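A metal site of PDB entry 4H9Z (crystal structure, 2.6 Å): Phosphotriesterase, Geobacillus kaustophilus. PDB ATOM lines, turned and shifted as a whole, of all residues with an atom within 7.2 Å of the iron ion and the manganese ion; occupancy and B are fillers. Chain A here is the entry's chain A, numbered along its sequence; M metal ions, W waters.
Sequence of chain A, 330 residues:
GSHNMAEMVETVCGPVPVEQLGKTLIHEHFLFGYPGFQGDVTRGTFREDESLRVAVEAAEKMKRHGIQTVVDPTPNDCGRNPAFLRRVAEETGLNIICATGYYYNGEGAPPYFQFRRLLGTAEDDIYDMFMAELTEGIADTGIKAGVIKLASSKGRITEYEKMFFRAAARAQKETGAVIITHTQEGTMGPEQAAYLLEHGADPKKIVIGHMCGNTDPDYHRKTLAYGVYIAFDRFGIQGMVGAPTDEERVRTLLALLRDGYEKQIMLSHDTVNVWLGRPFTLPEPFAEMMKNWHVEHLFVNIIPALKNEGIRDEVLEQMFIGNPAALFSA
The iron ion is bound by a ring nitrogen (NE2) of His 29, a ring nitrogen (NE2) of His 27, the side-chain carboxylate of Asp 270 and OQ1 of KCX 149.
Of the 23 residues printed, 4 come within 4 Å of the iron ion.
The nearest printed residue that does not touch the iron ion is His 210 (4.4 Å).
ND1 of His 29 sits at hydrogen-bond distance from OG1 of Thr 74.
The backbone carbonyl oxygen (O) of His 210 sits at hydrogen-bond distance from the side-chain hydroxyl (OG1) of Thr 183 (3.1 Å).
A ring nitrogen (ND1) of His 210 lies within hydrogen-bond range of the side-chain carboxylate (OD1) of Asp 233.
ND1 of His 27 is in hydrogen-bond range of OD2 of Asp 233 (3.5 Å).
The backbone NH (N) of Asp 270 lies within hydrogen-bond range of the backbone carbonyl oxygen (O) of Asp 233.
A ring nitrogen (ND1) of His 182 lies close to the side-chain hydroxyl (OH) of Tyr 103, 3.5 Å away.
The side-chain amide oxygen (OE1) of Gln 184 sits at hydrogen-bond distance from a ring nitrogen (NE2) of His 182, 2.7 Å away.
The backbone carbonyl oxygen (O) of Leu 150 lies within hydrogen-bond range of the backbone NH (N) of His 182 (2.8 Å).
The manganese ion is bound by a ring nitrogen (NE2) of His 210, OQ2 of KCX 149 and a ring nitrogen (ND1) of His 182.
The manganese ion has three donor atoms within binding distance.
Slightly farther from the manganese ion lies OH of Tyr 103 (2.9 Å).
Five residues have an atom within 4 Å of the manganese ion: Tyr 103, KCX 149, His 182, His 210 and Asp 270.
The nearest printed residue that does not touch the manganese ion is His 27 (4.3 Å).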
ATOM      1  N   HIS A  27      -8.957  27.668 -21.292  1.00  0.00           N
ATOM      2  CA  HIS A  27      -9.408  27.159 -20.003  1.00  0.00           C
ATOM      3  C   HIS A  27     -10.009  28.210 -19.096  1.00  0.00           C
ATOM      4  O   HIS A  27      -9.300  28.814 -18.302  1.00  0.00           O
ATOM      5  CB  HIS A  27      -8.216  26.515 -19.277  1.00  0.00           C
ATOM      6  CG  HIS A  27      -8.616  25.491 -18.270  1.00  0.00           C
ATOM      7  ND1 HIS A  27      -8.060  24.223 -18.237  1.00  0.00           N
ATOM      8  CD2 HIS A  27      -9.504  25.527 -17.254  1.00  0.00           C
ATOM      9  CE1 HIS A  27      -8.593  23.542 -17.248  1.00  0.00           C
ATOM     10  NE2 HIS A  27      -9.480  24.312 -16.641  1.00  0.00           N
ATOM     11  N   GLU A  28     -11.322  28.410 -19.197  1.00  0.00           N
ATOM     12  CA  GLU A  28     -12.049  29.295 -18.278  1.00  0.00           C
ATOM     13  C   GLU A  28     -13.417  28.692 -17.927  1.00  0.00           C
ATOM     14  O   GLU A  28     -14.064  28.092 -18.795  1.00  0.00           O
ATOM     15  CB  GLU A  28     -12.294  30.662 -18.917  1.00  0.00           C
ATOM     16  CG  GLU A  28     -11.114  31.300 -19.641  1.00  0.00           C
ATOM     17  CD  GLU A  28     -10.032  31.784 -18.714  1.00  0.00           C
ATOM     18  OE1 GLU A  28     -10.341  32.238 -17.583  1.00  0.00           O
ATOM     19  OE2 GLU A  28      -8.853  31.709 -19.122  1.00  0.00           O
ATOM     20  N   HIS A  29     -13.870  28.844 -16.683  1.00  0.00           N
ATOM     21  CA  HIS A  29     -15.227  28.389 -16.330  1.00  0.00           C
ATOM     22  C   HIS A  29     -16.224  29.551 -16.172  1.00  0.00           C
ATOM     23  O   HIS A  29     -15.953  30.515 -15.470  1.00  0.00           O
ATOM     24  CB  HIS A  29     -15.234  27.539 -15.055  1.00  0.00           C
ATOM     25  CG  HIS A  29     -14.259  26.405 -15.078  1.00  0.00           C
ATOM     26  ND1 HIS A  29     -14.609  25.136 -15.494  1.00  0.00           N
ATOM     27  CD2 HIS A  29     -12.956  26.345 -14.729  1.00  0.00           C
ATOM     28  CE1 HIS A  29     -13.560  24.339 -15.401  1.00  0.00           C
ATOM     29  NE2 HIS A  29     -12.540  25.054 -14.937  1.00  0.00           N
ATOM     30  N   PHE A  32     -19.037  26.952 -12.206  1.00  0.00           N
ATOM     31  CA  PHE A  32     -18.319  25.882 -11.535  1.00  0.00           C
ATOM     32  C   PHE A  32     -18.749  25.684 -10.074  1.00  0.00           C
ATOM     33  O   PHE A  32     -18.996  26.635  -9.327  1.00  0.00           O
ATOM     34  CB  PHE A  32     -16.800  26.065 -11.634  1.00  0.00           C
ATOM     35  CG  PHE A  32     -16.012  24.948 -10.999  1.00  0.00           C
ATOM     36  CD1 PHE A  32     -15.692  24.987  -9.640  1.00  0.00           C
ATOM     37  CD2 PHE A  32     -15.579  23.874 -11.745  1.00  0.00           C
ATOM     38  CE1 PHE A  32     -14.952  23.974  -9.070  1.00  0.00           C
ATOM     39  CE2 PHE A  32     -14.839  22.861 -11.176  1.00  0.00           C
ATOM     40  CZ  PHE A  32     -14.526  22.905  -9.834  1.00  0.00           C
ATOM     41  N   PRO A  73     -14.008  23.765 -19.897  1.00  0.00           N
ATOM     42  CA  PRO A  73     -13.757  22.359 -19.521  1.00  0.00           C
ATOM     43  C   PRO A  73     -14.403  21.950 -18.182  1.00  0.00           C
ATOM     44  O   PRO A  73     -13.891  21.078 -17.518  1.00  0.00           O
ATOM     45  CB  PRO A  73     -12.252  22.343 -19.351  1.00  0.00           C
ATOM     46  CG  PRO A  73     -11.961  23.717 -18.768  1.00  0.00           C
ATOM     47  CD  PRO A  73     -12.988  24.666 -19.330  1.00  0.00           C
ATOM     48  N   THR A  74     -15.503  22.585 -17.809  1.00  0.00           N
ATOM     49  CA  THR A  74     -16.166  22.278 -16.546  1.00  0.00           C
ATOM     50  C   THR A  74     -16.651  20.841 -16.599  1.00  0.00           C
ATOM     51  O   THR A  74     -17.432  20.473 -17.469  1.00  0.00           O
ATOM     52  CB  THR A  74     -17.351  23.237 -16.299  1.00  0.00           C
ATOM     53  OG1 THR A  74     -16.867  24.582 -16.194  1.00  0.00           O
ATOM     54  CG2 THR A  74     -18.090  22.878 -15.056  1.00  0.00           C
ATOM     55  N   PRO A  75     -16.165  19.995 -15.679  1.00  0.00           N
ATOM     56  CA  PRO A  75     -16.511  18.568 -15.767  1.00  0.00           C
ATOM     57  C   PRO A  75     -17.997  18.330 -15.497  1.00  0.00           C
ATOM     58  O   PRO A  75     -18.677  19.220 -14.997  1.00  0.00           O
ATOM     59  CB  PRO A  75     -15.646  17.925 -14.686  1.00  0.00           C
ATOM     60  CG  PRO A  75     -14.598  18.918 -14.368  1.00  0.00           C
ATOM     61  CD  PRO A  75     -15.212  20.266 -14.599  1.00  0.00           C
ATOM     62  N   TYR A 103     -14.150  15.042 -12.686  1.00  0.00           N
ATOM     63  CA  TYR A 103     -12.980  15.457 -11.971  1.00  0.00           C
ATOM     64  C   TYR A 103     -12.181  14.299 -11.405  1.00  0.00           C
ATOM     65  O   TYR A 103     -12.560  13.139 -11.510  1.00  0.00           O
ATOM     66  CB  TYR A 103     -13.344  16.431 -10.882  1.00  0.00           C
ATOM     67  CG  TYR A 103     -12.501  17.647 -10.903  1.00  0.00           C
ATOM     68  CD1 TYR A 103     -11.397  17.737 -11.721  1.00  0.00           C
ATOM     69  CD2 TYR A 103     -12.808  18.716 -10.104  1.00  0.00           C
ATOM     70  CE1 TYR A 103     -10.627  18.875 -11.736  1.00  0.00           C
ATOM     71  CE2 TYR A 103     -12.046  19.847 -10.129  1.00  0.00           C
ATOM     72  CZ  TYR A 103     -10.965  19.904 -10.948  1.00  0.00           C
ATOM     73  OH  TYR A 103     -10.259  21.013 -10.949  1.00  0.00           O
ATOM     74  N   TYR A 104     -11.009  14.628 -10.899  1.00  0.00           N
ATOM     75  CA  TYR A 104     -10.096  13.708 -10.256  1.00  0.00           C
ATOM     76  C   TYR A 104     -10.542  13.434  -8.842  1.00  0.00           C
ATOM     77  O   TYR A 104     -11.319  14.175  -8.303  1.00  0.00           O
ATOM     78  CB  TYR A 104      -8.660  14.255 -10.275  1.00  0.00           C
ATOM     79  CG  TYR A 104      -8.415  15.342  -9.293  1.00  0.00           C
ATOM     80  CD1 TYR A 104      -8.978  16.583  -9.450  1.00  0.00           C
ATOM     81  CD2 TYR A 104      -7.672  15.109  -8.183  1.00  0.00           C
ATOM     82  CE1 TYR A 104      -8.776  17.563  -8.524  1.00  0.00           C
ATOM     83  CE2 TYR A 104      -7.444  16.078  -7.269  1.00  0.00           C
ATOM     84  CZ  TYR A 104      -7.992  17.294  -7.449  1.00  0.00           C
ATOM     85  OH  TYR A 104      -7.759  18.203  -6.498  1.00  0.00           O
ATOM     86  N   GLU A 107     -11.010  16.247  -5.724  1.00  0.00           N
ATOM     87  CA  GLU A 107     -12.085  17.191  -5.868  1.00  0.00           C
ATOM     88  C   GLU A 107     -13.175  16.752  -6.878  1.00  0.00           C
ATOM     89  O   GLU A 107     -13.926  17.554  -7.368  1.00  0.00           O
ATOM     90  CB  GLU A 107     -11.541  18.593  -6.117  1.00  0.00           C
ATOM     91  CG  GLU A 107     -10.782  19.142  -4.930  1.00  0.00           C
ATOM     92  CD  GLU A 107     -10.338  20.566  -5.085  1.00  0.00           C
ATOM     93  OE1 GLU A 107      -9.727  20.879  -6.110  1.00  0.00           O
ATOM     94  OE2 GLU A 107     -10.603  21.376  -4.183  1.00  0.00           O
ATOM     95  N   KCX A 149     -12.365  16.080 -20.962  1.00  0.00           N
ATOM     96  CA  KCX A 149     -11.632  16.510 -19.786  1.00  0.00           C
ATOM     97  CB  KCX A 149     -12.497  17.402 -18.894  1.00  0.00           C
ATOM     98  CG  KCX A 149     -11.761  17.931 -17.638  1.00  0.00           C
ATOM     99  CD  KCX A 149     -10.593  18.804 -18.068  1.00  0.00           C
ATOM    100  CE  KCX A 149     -10.005  19.627 -16.925  1.00  0.00           C
ATOM    101  NZ  KCX A 149     -11.005  20.585 -16.393  1.00  0.00           N
ATOM    102  C   KCX A 149     -11.131  15.300 -18.989  1.00  0.00           C
ATOM    103  O   KCX A 149     -11.891  14.366 -18.684  1.00  0.00           O
ATOM    104  CX  KCX A 149     -10.687  21.127 -15.229  1.00  0.00           C
ATOM    105  OQ1 KCX A 149     -11.449  21.923 -14.648  1.00  0.00           O
ATOM    106  OQ2 KCX A 149      -9.597  20.805 -14.744  1.00  0.00           O
ATOM    107  N   LEU A 150      -9.839  15.336 -18.666  1.00  0.00           N
ATOM    108  CA  LEU A 150      -9.203  14.327 -17.841  1.00  0.00           C
ATOM    109  C   LEU A 150      -8.497  14.987 -16.661  1.00  0.00           C
ATOM    110  O   LEU A 150      -8.004  16.102 -16.782  1.00  0.00           O
ATOM    111  CB  LEU A 150      -8.170  13.553 -18.663  1.00  0.00           C
ATOM    112  CG  LEU A 150      -8.665  12.546 -19.701  1.00  0.00           C
ATOM    113  CD1 LEU A 150      -7.498  11.683 -20.146  1.00  0.00           C
ATOM    114  CD2 LEU A 150      -9.801  11.672 -19.174  1.00  0.00           C
ATOM    115  N   ALA A 151      -8.446  14.303 -15.526  1.00  0.00           N
ATOM    116  CA  ALA A 151      -7.697  14.793 -14.362  1.00  0.00           C
ATOM    117  C   ALA A 151      -6.946  13.696 -13.568  1.00  0.00           C
ATOM    118  O   ALA A 151      -7.414  12.560 -13.450  1.00  0.00           O
ATOM    119  CB  ALA A 151      -8.593  15.567 -13.468  1.00  0.00           C
ATOM    120  N   THR A 181      -6.518  18.275 -20.091  1.00  0.00           N
ATOM    121  CA  THR A 181      -6.303  17.635 -18.806  1.00  0.00           C
ATOM    122  C   THR A 181      -6.036  18.618 -17.662  1.00  0.00           C
ATOM    123  O   THR A 181      -5.740  19.805 -17.871  1.00  0.00           O
ATOM    124  CB  THR A 181      -5.111  16.661 -18.842  1.00  0.00           C
ATOM    125  OG1 THR A 181      -3.893  17.404 -18.789  1.00  0.00           O
ATOM    126  CG2 THR A 181      -5.137  15.808 -20.101  1.00  0.00           C
ATOM    127  N   HIS A 182      -6.143  18.102 -16.451  1.00  0.00           N
ATOM    128  CA  HIS A 182      -5.857  18.827 -15.228  1.00  0.00           C
ATOM    129  C   HIS A 182      -4.700  18.116 -14.551  1.00  0.00           C
ATOM    130  O   HIS A 182      -4.730  16.889 -14.413  1.00  0.00           O
ATOM    131  CB  HIS A 182      -7.090  18.793 -14.329  1.00  0.00           C
ATOM    132  CG  HIS A 182      -6.802  18.966 -12.868  1.00  0.00           C
ATOM    133  ND1 HIS A 182      -7.152  20.109 -12.177  1.00  0.00           N
ATOM    134  CD2 HIS A 182      -6.238  18.132 -11.962  1.00  0.00           C
ATOM    135  CE1 HIS A 182      -6.800  19.970 -10.907  1.00  0.00           C
ATOM    136  NE2 HIS A 182      -6.234  18.792 -10.745  1.00  0.00           N
ATOM    137  N   THR A 183      -3.677  18.859 -14.157  1.00  0.00           N
ATOM    138  CA  THR A 183      -2.640  18.258 -13.322  1.00  0.00           C
ATOM    139  C   THR A 183      -2.746  18.871 -11.948  1.00  0.00           C
ATOM    140  O   THR A 183      -3.103  20.044 -11.792  1.00  0.00           O
ATOM    141  CB  THR A 183      -1.210  18.443 -13.880  1.00  0.00           C
ATOM    142  OG1 THR A 183      -0.909  19.847 -14.002  1.00  0.00           O
ATOM    143  CG2 THR A 183      -1.040  17.756 -15.230  1.00  0.00           C
ATOM    144  N   GLN A 184      -2.459  18.046 -10.944  1.00  0.00           N
ATOM    145  CA  GLN A 184      -2.579  18.502  -9.573  1.00  0.00           C
ATOM    146  C   GLN A 184      -1.215  18.942  -9.039  1.00  0.00           C
ATOM    147  O   GLN A 184      -0.263  18.148  -8.988  1.00  0.00           O
ATOM    148  CB  GLN A 184      -3.174  17.401  -8.704  1.00  0.00           C
ATOM    149  CG  GLN A 184      -3.508  17.856  -7.292  1.00  0.00           C
ATOM    150  CD  GLN A 184      -4.563  18.967  -7.247  1.00  0.00           C
ATOM    151  OE1 GLN A 184      -5.253  19.251  -8.231  1.00  0.00           O
ATOM    152  NE2 GLN A 184      -4.679  19.598  -6.094  1.00  0.00           N
ATOM    153  N   HIS A 210      -2.514  22.963 -16.394  1.00  0.00           N
ATOM    154  CA  HIS A 210      -1.962  23.359 -15.099  1.00  0.00           C
ATOM    155  C   HIS A 210      -0.465  23.127 -15.025  1.00  0.00           C
ATOM    156  O   HIS A 210       0.068  22.801 -13.943  1.00  0.00           O
ATOM    157  CB  HIS A 210      -2.656  22.611 -13.972  1.00  0.00           C
ATOM    158  CG  HIS A 210      -4.142  22.794 -13.953  1.00  0.00           C
ATOM    159  ND1 HIS A 210      -4.777  23.789 -14.662  1.00  0.00           N
ATOM    160  CD2 HIS A 210      -5.111  22.109 -13.315  1.00  0.00           C
ATOM    161  CE1 HIS A 210      -6.073  23.708 -14.461  1.00  0.00           C
ATOM    162  NE2 HIS A 210      -6.305  22.689 -13.654  1.00  0.00           N
ATOM    163  N   ASP A 233      -2.483  27.684 -17.586  1.00  0.00           N
ATOM    164  CA  ASP A 233      -3.884  28.070 -17.653  1.00  0.00           C
ATOM    165  C   ASP A 233      -4.399  28.579 -16.328  1.00  0.00           C
ATOM    166  O   ASP A 233      -5.606  28.679 -16.133  1.00  0.00           O
ATOM    167  CB  ASP A 233      -4.735  26.894 -18.153  1.00  0.00           C
ATOM    168  CG  ASP A 233      -4.444  25.594 -17.415  1.00  0.00           C
ATOM    169  OD1 ASP A 233      -4.070  25.641 -16.225  1.00  0.00           O
ATOM    170  OD2 ASP A 233      -4.588  24.522 -18.026  1.00  0.00           O
ATOM    171  N   ARG A 234      -3.485  28.886 -15.421  1.00  0.00           N
ATOM    172  CA  ARG A 234      -3.880  29.310 -14.094  1.00  0.00           C
ATOM    173  C   ARG A 234      -3.331  30.683 -13.710  1.00  0.00           C
ATOM    174  O   ARG A 234      -3.042  30.933 -12.546  1.00  0.00           O
ATOM    175  CB  ARG A 234      -3.512  28.250 -13.048  1.00  0.00           C
ATOM    176  CG  ARG A 234      -4.632  27.280 -12.714  1.00  0.00           C
ATOM    177  CD  ARG A 234      -4.159  26.197 -11.776  1.00  0.00           C
ATOM    178  NE  ARG A 234      -5.248  25.622 -10.980  1.00  0.00           N
ATOM    179  CZ  ARG A 234      -5.116  24.549 -10.193  1.00  0.00           C
ATOM    180  NH1 ARG A 234      -3.947  23.929 -10.085  1.00  0.00           N
ATOM    181  NH2 ARG A 234      -6.169  24.092  -9.520  1.00  0.00           N
ATOM    182  N   ASP A 270      -8.110  29.916 -15.889  1.00  0.00           N
ATOM    183  CA  ASP A 270      -8.913  28.920 -15.160  1.00  0.00           C
ATOM    184  C   ASP A 270      -9.915  29.615 -14.227  1.00  0.00           C
ATOM    185  O   ASP A 270     -10.105  29.175 -13.087  1.00  0.00           O
ATOM    186  CB  ASP A 270      -8.002  27.953 -14.376  1.00  0.00           C
ATOM    187  CG  ASP A 270      -8.726  26.730 -13.876  1.00  0.00           C
ATOM    188  OD1 ASP A 270      -9.971  26.698 -14.018  1.00  0.00           O
ATOM    189  OD2 ASP A 270      -8.056  25.795 -13.349  1.00  0.00           O
ATOM    190  N   THR A 271     -10.548  30.691 -14.687  1.00  0.00           N
ATOM    191  CA  THR A 271     -11.470  31.424 -13.816  1.00  0.00           C
ATOM    192  C   THR A 271     -12.750  30.647 -13.616  1.00  0.00           C
ATOM    193  O   THR A 271     -13.074  29.733 -14.374  1.00  0.00           O
ATOM    194  CB  THR A 271     -11.898  32.824 -14.349  1.00  0.00           C
ATOM    195  OG1 THR A 271     -12.687  32.681 -15.530  1.00  0.00           O
ATOM    196  CG2 THR A 271     -10.709  33.725 -14.626  1.00  0.00           C
ATOM    197  N   VAL A 272     -13.455  31.047 -12.548  1.00  0.00           N
ATOM    198  CA  VAL A 272     -14.816  30.642 -12.245  1.00  0.00           C
ATOM    199  C   VAL A 272     -15.636  31.927 -12.106  1.00  0.00           C
ATOM    200  O   VAL A 272     -15.614  32.600 -11.066  1.00  0.00           O
ATOM    201  CB  VAL A 272     -14.896  29.831 -10.935  1.00  0.00           C
ATOM    202  CG1 VAL A 272     -16.347  29.465 -10.634  1.00  0.00           C
ATOM    203  CG2 VAL A 272     -14.052  28.597 -11.037  1.00  0.00           C
HETATM  204 FE    FE M   1     -10.425  24.299 -14.386  1.00  0.00          FE
HETATM  205 MN    MN M   2      -8.533  22.157 -13.006  1.00  0.00          MN
HETATM  206  O   HOH W   1     -10.997  24.172 -11.560  1.00  0.00           O
